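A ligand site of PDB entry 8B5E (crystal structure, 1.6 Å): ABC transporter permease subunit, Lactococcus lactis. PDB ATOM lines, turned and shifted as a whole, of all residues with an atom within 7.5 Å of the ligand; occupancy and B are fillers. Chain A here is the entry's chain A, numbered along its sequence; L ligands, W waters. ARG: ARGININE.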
ATOM      1  N   ASP A   9      31.928 -22.566 -14.569  1.00  0.00           N
ATOM      2  CA  ASP A   9      32.274 -21.607 -13.533  1.00  0.00           C
ATOM      3  C   ASP A   9      33.079 -22.326 -12.455  1.00  0.00           C
ATOM      4  O   ASP A   9      33.105 -23.562 -12.377  1.00  0.00           O
ATOM      5  CB  ASP A   9      31.036 -20.907 -12.940  1.00  0.00           C
ATOM      6  CG  ASP A   9      31.360 -19.726 -12.047  1.00  0.00           C
ATOM      7  OD1 ASP A   9      32.104 -18.814 -12.489  1.00  0.00           O
ATOM      8  OD2 ASP A   9      30.986 -19.765 -10.880  1.00  0.00           O
ATOM      9  N   SER A  10      33.704 -21.541 -11.574  1.00  0.00           N
ATOM     10  CA  SER A  10      34.585 -22.099 -10.554  1.00  0.00           C
ATOM     11  C   SER A  10      33.878 -22.248  -9.210  1.00  0.00           C
ATOM     12  O   SER A  10      34.332 -23.027  -8.360  1.00  0.00           O
ATOM     13  CB  SER A  10      35.833 -21.244 -10.427  1.00  0.00           C
ATOM     14  OG  SER A  10      35.465 -19.904 -10.174  1.00  0.00           O
ATOM     15  N   SER A  11      32.754 -21.556  -9.029  1.00  0.00           N
ATOM     16  CA  SER A  11      31.976 -21.669  -7.805  1.00  0.00           C
ATOM     17  C   SER A  11      30.563 -21.117  -7.994  1.00  0.00           C
ATOM     18  O   SER A  11      30.345 -19.899  -7.859  1.00  0.00           O
ATOM     19  CB  SER A  11      32.695 -20.966  -6.671  1.00  0.00           C
ATOM     20  OG  SER A  11      31.958 -21.059  -5.456  1.00  0.00           O
ATOM     21  N   TYR A  12      29.610 -22.005  -8.274  1.00  0.00           N
ATOM     22  CA  TYR A  12      28.220 -21.633  -8.510  1.00  0.00           C
ATOM     23  C   TYR A  12      27.339 -22.788  -8.014  1.00  0.00           C
ATOM     24  O   TYR A  12      26.670 -23.428  -8.834  1.00  0.00           O
ATOM     25  CB  TYR A  12      28.010 -21.309  -9.992  1.00  0.00           C
ATOM     26  CG  TYR A  12      26.675 -20.755 -10.419  1.00  0.00           C
ATOM     27  CD1 TYR A  12      25.770 -20.208  -9.521  1.00  0.00           C
ATOM     28  CD2 TYR A  12      26.332 -20.736 -11.770  1.00  0.00           C
ATOM     29  CE1 TYR A  12      24.571 -19.643  -9.943  1.00  0.00           C
ATOM     30  CE2 TYR A  12      25.135 -20.182 -12.211  1.00  0.00           C
ATOM     31  CZ  TYR A  12      24.250 -19.634 -11.302  1.00  0.00           C
ATOM     32  OH  TYR A  12      23.067 -19.077 -11.785  1.00  0.00           O
ATOM     33  N   ALA A  13      27.368 -23.042  -6.698  1.00  0.00           N
ATOM     34  CA  ALA A  13      26.574 -24.096  -6.103  1.00  0.00           C
ATOM     35  C   ALA A  13      25.108 -23.723  -6.237  1.00  0.00           C
ATOM     36  O   ALA A  13      24.740 -22.571  -5.993  1.00  0.00           O
ATOM     37  CB  ALA A  13      26.955 -24.302  -4.640  1.00  0.00           C
ATOM     38  N   PHE A  15      25.132 -25.674  -9.124  1.00  0.00           N
ATOM     39  CA  PHE A  15      25.415 -26.055 -10.510  1.00  0.00           C
ATOM     40  C   PHE A  15      26.813 -26.651 -10.661  1.00  0.00           C
ATOM     41  O   PHE A  15      26.968 -27.719 -11.232  1.00  0.00           O
ATOM     42  CB  PHE A  15      25.152 -24.835 -11.399  1.00  0.00           C
ATOM     43  CG  PHE A  15      23.707 -24.423 -11.362  1.00  0.00           C
ATOM     44  CD1 PHE A  15      22.731 -25.169 -12.014  1.00  0.00           C
ATOM     45  CD2 PHE A  15      23.298 -23.313 -10.629  1.00  0.00           C
ATOM     46  CE1 PHE A  15      21.395 -24.811 -11.926  1.00  0.00           C
ATOM     47  CE2 PHE A  15      21.965 -22.946 -10.566  1.00  0.00           C
ATOM     48  CZ  PHE A  15      21.015 -23.707 -11.197  1.00  0.00           C
ATOM     49  N   GLU A  16      27.845 -25.940 -10.197  1.00  0.00           N
ATOM     50  CA  GLU A  16      29.213 -26.470 -10.146  1.00  0.00           C
ATOM     51  C   GLU A  16      29.917 -25.858  -8.933  1.00  0.00           C
ATOM     52  O   GLU A  16      29.810 -24.643  -8.704  1.00  0.00           O
ATOM     53  CB  GLU A  16      30.000 -26.206 -11.426  1.00  0.00           C
ATOM     54  CG  GLU A  16      29.922 -24.766 -11.957  1.00  0.00           C
ATOM     55  CD  GLU A  16      28.702 -24.449 -12.811  1.00  0.00           C
ATOM     56  OE1 GLU A  16      28.071 -25.445 -13.298  1.00  0.00           O
ATOM     57  OE2 GLU A  16      28.379 -23.237 -13.026  1.00  0.00           O
ATOM     58  N   PHE A  50      33.121 -18.312 -15.170  1.00  0.00           N
ATOM     59  CA  PHE A  50      32.177 -18.048 -16.257  1.00  0.00           C
ATOM     60  C   PHE A  50      32.799 -17.154 -17.338  1.00  0.00           C
ATOM     61  O   PHE A  50      32.753 -17.508 -18.502  1.00  0.00           O
ATOM     62  CB  PHE A  50      30.870 -17.449 -15.714  1.00  0.00           C
ATOM     63  CG  PHE A  50      29.799 -17.215 -16.742  1.00  0.00           C
ATOM     64  CD1 PHE A  50      29.206 -18.272 -17.429  1.00  0.00           C
ATOM     65  CD2 PHE A  50      29.398 -15.935 -17.044  1.00  0.00           C
ATOM     66  CE1 PHE A  50      28.221 -18.025 -18.385  1.00  0.00           C
ATOM     67  CE2 PHE A  50      28.423 -15.697 -17.978  1.00  0.00           C
ATOM     68  CZ  PHE A  50      27.828 -16.743 -18.646  1.00  0.00           C
ATOM     69  N   ALA A  67      27.229 -23.744 -17.317  1.00  0.00           N
ATOM     70  CA  ALA A  67      27.543 -22.900 -16.154  1.00  0.00           C
ATOM     71  C   ALA A  67      26.311 -22.089 -15.741  1.00  0.00           C
ATOM     72  O   ALA A  67      26.393 -20.859 -15.650  1.00  0.00           O
ATOM     73  CB  ALA A  67      28.705 -21.994 -16.511  1.00  0.00           C
ATOM     74  N   GLY A  68      25.172 -22.756 -15.542  1.00  0.00           N
ATOM     75  CA  GLY A  68      23.933 -22.064 -15.221  1.00  0.00           C
ATOM     76  C   GLY A  68      23.731 -20.831 -16.102  1.00  0.00           C
ATOM     77  O   GLY A  68      23.427 -19.761 -15.587  1.00  0.00           O
ATOM     78  N   MET A  69      23.907 -21.024 -17.421  1.00  0.00           N
ATOM     79  CA  MET A  69      23.966 -19.902 -18.345  1.00  0.00           C
ATOM     80  C   MET A  69      22.581 -19.584 -18.929  1.00  0.00           C
ATOM     81  O   MET A  69      22.012 -20.381 -19.683  1.00  0.00           O
ATOM     82  CB  MET A  69      24.972 -20.206 -19.456  1.00  0.00           C
ATOM     83  CG  MET A  69      25.169 -19.072 -20.474  1.00  0.00           C
ATOM     84  SD  MET A  69      26.485 -19.459 -21.609  1.00  0.00           S
ATOM     85  CE  MET A  69      26.504 -18.039 -22.681  1.00  0.00           C
ATOM     86  N   THR A  70      22.045 -18.414 -18.585  1.00  0.00           N
ATOM     87  CA  THR A  70      20.742 -17.975 -19.056  1.00  0.00           C
ATOM     88  C   THR A  70      20.733 -17.829 -20.578  1.00  0.00           C
ATOM     89  O   THR A  70      21.645 -17.229 -21.161  1.00  0.00           O
ATOM     90  CB  THR A  70      20.349 -16.627 -18.399  1.00  0.00           C
ATOM     91  OG1 THR A  70      20.556 -16.710 -16.980  1.00  0.00           O
ATOM     92  CG2 THR A  70      18.913 -16.260 -18.698  1.00  0.00           C
ATOM     93  N   ILE A  71      19.700 -18.388 -21.230  1.00  0.00           N
ATOM     94  CA  ILE A  71      19.521 -18.195 -22.664  1.00  0.00           C
ATOM     95  C   ILE A  71      18.922 -16.804 -22.897  1.00  0.00           C
ATOM     96  O   ILE A  71      17.832 -16.549 -22.415  1.00  0.00           O
ATOM     97  CB  ILE A  71      18.625 -19.323 -23.246  1.00  0.00           C
ATOM     98  CG1 ILE A  71      19.240 -20.721 -23.013  1.00  0.00           C
ATOM     99  CG2 ILE A  71      18.346 -19.071 -24.728  1.00  0.00           C
ATOM    100  CD1 ILE A  71      18.273 -21.886 -23.101  1.00  0.00           C
ATOM    101  N   THR A  72      19.615 -15.912 -23.623  1.00  0.00           N
ATOM    102  CA  THR A  72      19.124 -14.564 -23.884  1.00  0.00           C
ATOM    103  C   THR A  72      19.296 -14.257 -25.361  1.00  0.00           C
ATOM    104  O   THR A  72      20.169 -14.815 -26.000  1.00  0.00           O
ATOM    105  CB  THR A  72      19.876 -13.500 -23.053  1.00  0.00           C
ATOM    106  OG1 THR A  72      21.181 -13.287 -23.584  1.00  0.00           O
ATOM    107  CG2 THR A  72      19.978 -13.873 -21.593  1.00  0.00           C
ATOM    108  N   ARG A  75      22.784 -13.070 -26.110  1.00  0.00           N
ATOM    109  CA  ARG A  75      23.732 -14.184 -26.188  1.00  0.00           C
ATOM    110  C   ARG A  75      23.560 -14.976 -27.484  1.00  0.00           C
ATOM    111  O   ARG A  75      24.549 -15.438 -28.029  1.00  0.00           O
ATOM    112  CB  ARG A  75      23.606 -15.074 -24.952  1.00  0.00           C
ATOM    113  CG  ARG A  75      24.184 -14.375 -23.728  1.00  0.00           C
ATOM    114  CD  ARG A  75      23.841 -15.037 -22.421  1.00  0.00           C
ATOM    115  NE  ARG A  75      24.610 -14.439 -21.325  1.00  0.00           N
ATOM    116  CZ  ARG A  75      24.492 -14.814 -20.048  1.00  0.00           C
ATOM    117  NH1 ARG A  75      23.663 -15.782 -19.710  1.00  0.00           N
ATOM    118  NH2 ARG A  75      25.182 -14.199 -19.120  1.00  0.00           N
ATOM    119  N   SER A  88      15.484 -21.559 -13.702  1.00  0.00           N
ATOM    120  CA  SER A  88      15.617 -20.984 -12.364  1.00  0.00           C
ATOM    121  C   SER A  88      14.568 -19.898 -12.139  1.00  0.00           C
ATOM    122  O   SER A  88      13.749 -19.572 -13.013  1.00  0.00           O
ATOM    123  CB  SER A  88      17.033 -20.439 -12.156  1.00  0.00           C
ATOM    124  OG  SER A  88      17.256 -20.108 -10.787  1.00  0.00           O
ATOM    125  N   LYS A 114      23.349 -10.405  -3.747  1.00  0.00           N
ATOM    126  CA  LYS A 114      24.734 -10.456  -4.195  1.00  0.00           C
ATOM    127  C   LYS A 114      24.952  -9.423  -5.308  1.00  0.00           C
ATOM    128  O   LYS A 114      24.137  -9.320  -6.212  1.00  0.00           O
ATOM    129  CB  LYS A 114      25.080 -11.868  -4.693  1.00  0.00           C
ATOM    130  CG  LYS A 114      25.147 -12.925  -3.593  1.00  0.00           C
ATOM    131  CD  LYS A 114      25.644 -14.291  -4.018  1.00  0.00           C
ATOM    132  CE  LYS A 114      24.577 -15.118  -4.692  1.00  0.00           C
ATOM    133  NZ  LYS A 114      24.721 -16.554  -4.309  1.00  0.00           N
ATOM    134  N   GLY A 116      26.009  -7.690  -8.647  1.00  0.00           N
ATOM    135  CA  GLY A 116      26.169  -8.110 -10.030  1.00  0.00           C
ATOM    136  C   GLY A 116      25.267  -9.277 -10.413  1.00  0.00           C
ATOM    137  O   GLY A 116      25.616 -10.022 -11.334  1.00  0.00           O
ATOM    138  N   THR A 117      24.113  -9.430  -9.727  1.00  0.00           N
ATOM    139  CA  THR A 117      23.201 -10.529  -9.995  1.00  0.00           C
ATOM    140  C   THR A 117      21.830 -10.015 -10.427  1.00  0.00           C
ATOM    141  O   THR A 117      21.461  -8.882 -10.152  1.00  0.00           O
ATOM    142  CB  THR A 117      22.995 -11.431  -8.754  1.00  0.00           C
ATOM    143  OG1 THR A 117      22.327 -10.639  -7.762  1.00  0.00           O
ATOM    144  CG2 THR A 117      24.272 -12.059  -8.258  1.00  0.00           C
ATOM    145  N   ALA A 118      21.064 -10.890 -11.122  1.00  0.00           N
ATOM    146  CA  ALA A 118      19.663 -10.647 -11.423  1.00  0.00           C
ATOM    147  C   ALA A 118      18.854 -10.292 -10.176  1.00  0.00           C
ATOM    148  O   ALA A 118      17.938  -9.472 -10.256  1.00  0.00           O
ATOM    149  CB  ALA A 118      19.090 -11.862 -12.120  1.00  0.00           C
ATOM    150  N   ASP A 157      17.754 -14.400  -3.818  1.00  0.00           N
ATOM    151  CA  ASP A 157      18.689 -15.252  -4.534  1.00  0.00           C
ATOM    152  C   ASP A 157      17.865 -16.206  -5.405  1.00  0.00           C
ATOM    153  O   ASP A 157      16.646 -16.103  -5.437  1.00  0.00           O
ATOM    154  CB  ASP A 157      19.558 -16.043  -3.549  1.00  0.00           C
ATOM    155  CG  ASP A 157      20.955 -16.402  -4.048  1.00  0.00           C
ATOM    156  OD1 ASP A 157      21.149 -16.638  -5.287  1.00  0.00           O
ATOM    157  OD2 ASP A 157      21.848 -16.513  -3.180  1.00  0.00           O
ATOM    158  N   GLU A 158      18.548 -17.117  -6.102  1.00  0.00           N
ATOM    159  CA  GLU A 158      17.883 -18.112  -6.946  1.00  0.00           C
ATOM    160  C   GLU A 158      17.323 -19.244  -6.088  1.00  0.00           C
ATOM    161  O   GLU A 158      17.963 -19.692  -5.137  1.00  0.00           O
ATOM    162  CB  GLU A 158      18.888 -18.691  -7.931  1.00  0.00           C
ATOM    163  CG  GLU A 158      19.530 -17.676  -8.864  1.00  0.00           C
ATOM    164  CD  GLU A 158      20.408 -18.347  -9.889  1.00  0.00           C
ATOM    165  OE1 GLU A 158      21.594 -17.919 -10.046  1.00  0.00           O
ATOM    166  OE2 GLU A 158      19.909 -19.328 -10.524  1.00  0.00           O
ATOM    167  N   VAL A 161      19.712 -22.148  -5.487  1.00  0.00           N
ATOM    168  CA  VAL A 161      20.821 -21.815  -4.607  1.00  0.00           C
ATOM    169  C   VAL A 161      20.338 -21.880  -3.148  1.00  0.00           C
ATOM    170  O   VAL A 161      21.007 -22.468  -2.320  1.00  0.00           O
ATOM    171  CB  VAL A 161      21.407 -20.436  -4.979  1.00  0.00           C
ATOM    172  CG1 VAL A 161      22.404 -19.922  -3.944  1.00  0.00           C
ATOM    173  CG2 VAL A 161      22.033 -20.459  -6.363  1.00  0.00           C
ATOM    174  N   LEU A 181      12.949 -16.497 -14.127  1.00  0.00           N
ATOM    175  CA  LEU A 181      14.051 -15.957 -14.930  1.00  0.00           C
ATOM    176  C   LEU A 181      13.851 -16.439 -16.359  1.00  0.00           C
ATOM    177  O   LEU A 181      14.216 -17.570 -16.688  1.00  0.00           O
ATOM    178  CB  LEU A 181      15.385 -16.408 -14.335  1.00  0.00           C
ATOM    179  CG  LEU A 181      15.744 -15.790 -12.988  1.00  0.00           C
ATOM    180  CD1 LEU A 181      16.869 -16.549 -12.307  1.00  0.00           C
ATOM    181  CD2 LEU A 181      16.158 -14.340 -13.171  1.00  0.00           C
ATOM    182  N   GLY A 184      15.686 -19.788 -19.198  1.00  0.00           N
ATOM    183  CA  GLY A 184      16.231 -21.051 -18.728  1.00  0.00           C
ATOM    184  C   GLY A 184      17.740 -21.114 -18.944  1.00  0.00           C
ATOM    185  O   GLY A 184      18.320 -20.251 -19.616  1.00  0.00           O
ATOM    186  N   TYR A 185      18.370 -22.118 -18.317  1.00  0.00           N
ATOM    187  CA  TYR A 185      19.797 -22.311 -18.443  1.00  0.00           C
ATOM    188  C   TYR A 185      20.049 -23.357 -19.524  1.00  0.00           C
ATOM    189  O   TYR A 185      19.361 -24.369 -19.553  1.00  0.00           O
ATOM    190  CB  TYR A 185      20.357 -22.805 -17.087  1.00  0.00           C
ATOM    191  CG  TYR A 185      20.300 -21.772 -15.993  1.00  0.00           C
ATOM    192  CD1 TYR A 185      20.064 -20.433 -16.306  1.00  0.00           C
ATOM    193  CD2 TYR A 185      20.491 -22.086 -14.663  1.00  0.00           C
ATOM    194  CE1 TYR A 185      20.036 -19.454 -15.333  1.00  0.00           C
ATOM    195  CE2 TYR A 185      20.480 -21.098 -13.685  1.00  0.00           C
ATOM    196  CZ  TYR A 185      20.213 -19.786 -14.005  1.00  0.00           C
ATOM    197  OH  TYR A 185      20.191 -18.777 -13.029  1.00  0.00           O
HETATM  198  N   ARG L   1      23.023 -17.343 -14.295  1.00  0.00           N
HETATM  199  CA  ARG L   1      24.155 -16.416 -14.543  1.00  0.00           C
HETATM  200  C   ARG L   1      23.991 -15.821 -15.946  1.00  0.00           C
HETATM  201  O   ARG L   1      24.594 -14.809 -16.230  1.00  0.00           O
HETATM  202  CB  ARG L   1      25.497 -17.150 -14.473  1.00  0.00           C
HETATM  203  CG  ARG L   1      26.514 -16.548 -13.524  1.00  0.00           C
HETATM  204  CD  ARG L   1      26.214 -16.833 -12.061  1.00  0.00           C
HETATM  205  NE  ARG L   1      27.333 -17.367 -11.289  1.00  0.00           N
HETATM  206  CZ  ARG L   1      27.350 -17.458  -9.960  1.00  0.00           C
HETATM  207  NH1 ARG L   1      28.479 -17.711  -9.311  1.00  0.00           N
HETATM  208  NH2 ARG L   1      26.235 -17.301  -9.267  1.00  0.00           N
HETATM  209  OXT ARG L   1      23.302 -16.403 -16.702  1.00  0.00           O
HETATM  210  O   HOH W   1      20.434 -15.980 -13.488  1.00  0.00           O
HETATM  211  O   HOH W   2      23.132 -15.958  -8.891  1.00  0.00           O
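O of Gly 68 lies within hydrogen-bond range of N of the ligand. OXT of the ligand lies within hydrogen-bond range of N of Thr 70 (3.0 Å). The side-chain hydroxyl (OG1) of Thr 70 is in hydrogen-bond range of an oxygen (OXT) of the ligand, at 2.8 Å. The side-chain hydroxyl of Tyr 12 lies within hydrogen-bond range of a nitrogen (N) of the ligand, at 3.1 Å. The guanidinium group of Arg 75 is in salt-bridge range of an oxygen (O) of the ligand, 3.0 Å away. The backbone carbonyl oxygen (O) of Ser 11 lies within hydrogen-bond range of a nitrogen (NH1) of the ligand (3.2 Å). A nitrogen (N) of the ligand lies within hydrogen-bond range of the side-chain hydroxyl (OH) of Tyr 185 (3.4 Å). A nitrogen (NH1) of the ligand lies within salt-bridge range of the side-chain carboxylate (OD2) of Asp 9 (3.6 Å).
O of Thr 70 lies within hydrogen-bond range of NH1 of Arg 75 (2.9 Å). OH of Tyr 12 sits at hydrogen-bond distance from OH of Tyr 185 (3.1 Å). The side-chain carboxylate (OE1) of Glu 158 sits at hydrogen-bond distance from the side-chain hydroxyl (OH) of Tyr 12 (2.6 Å). N of Arg 75 lies within hydrogen-bond range of OG1 of Thr 72, 3.0 Å away. The backbone NH (N) of Ser 11 lies within hydrogen-bond range of the side-chain carboxylate (OD2) of Asp 9 (3.1 Å). The side-chain carboxylate (OE2) of Glu 158 lies within hydrogen-bond range of the side-chain hydroxyl (OH) of Tyr 185, 2.6 Å away. N of Phe 50 is in hydrogen-bond range of OD1 of Asp 9 (2.9 Å).
Merely in contact with the ligand: Met 69 (3.9 Å) and Ala 67 (3.99 Å). Hydrophobic or aromatic side chains that line the ligand: Tyr 12 and Tyr 185. Within 4 Å of the ligand: Asp 9, Ser 11, Tyr 12, Ala 67, Gly 68, Met 69, Thr 70, Arg 75 and Tyr 185. Along chain A the residues within 4 Å of the ligand span positions 9 to 185. The nearest printed residue that does not touch the ligand is Phe 50 (4.3 Å).
Water W1 lies within hydrogen-bond range of OH of Tyr 185 (2.8 Å) and N of the ligand (3.0 Å). Water W2 bridges OE1 of Glu 158 (2.7 Å) and NH2 of the ligand (3.4 Å).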
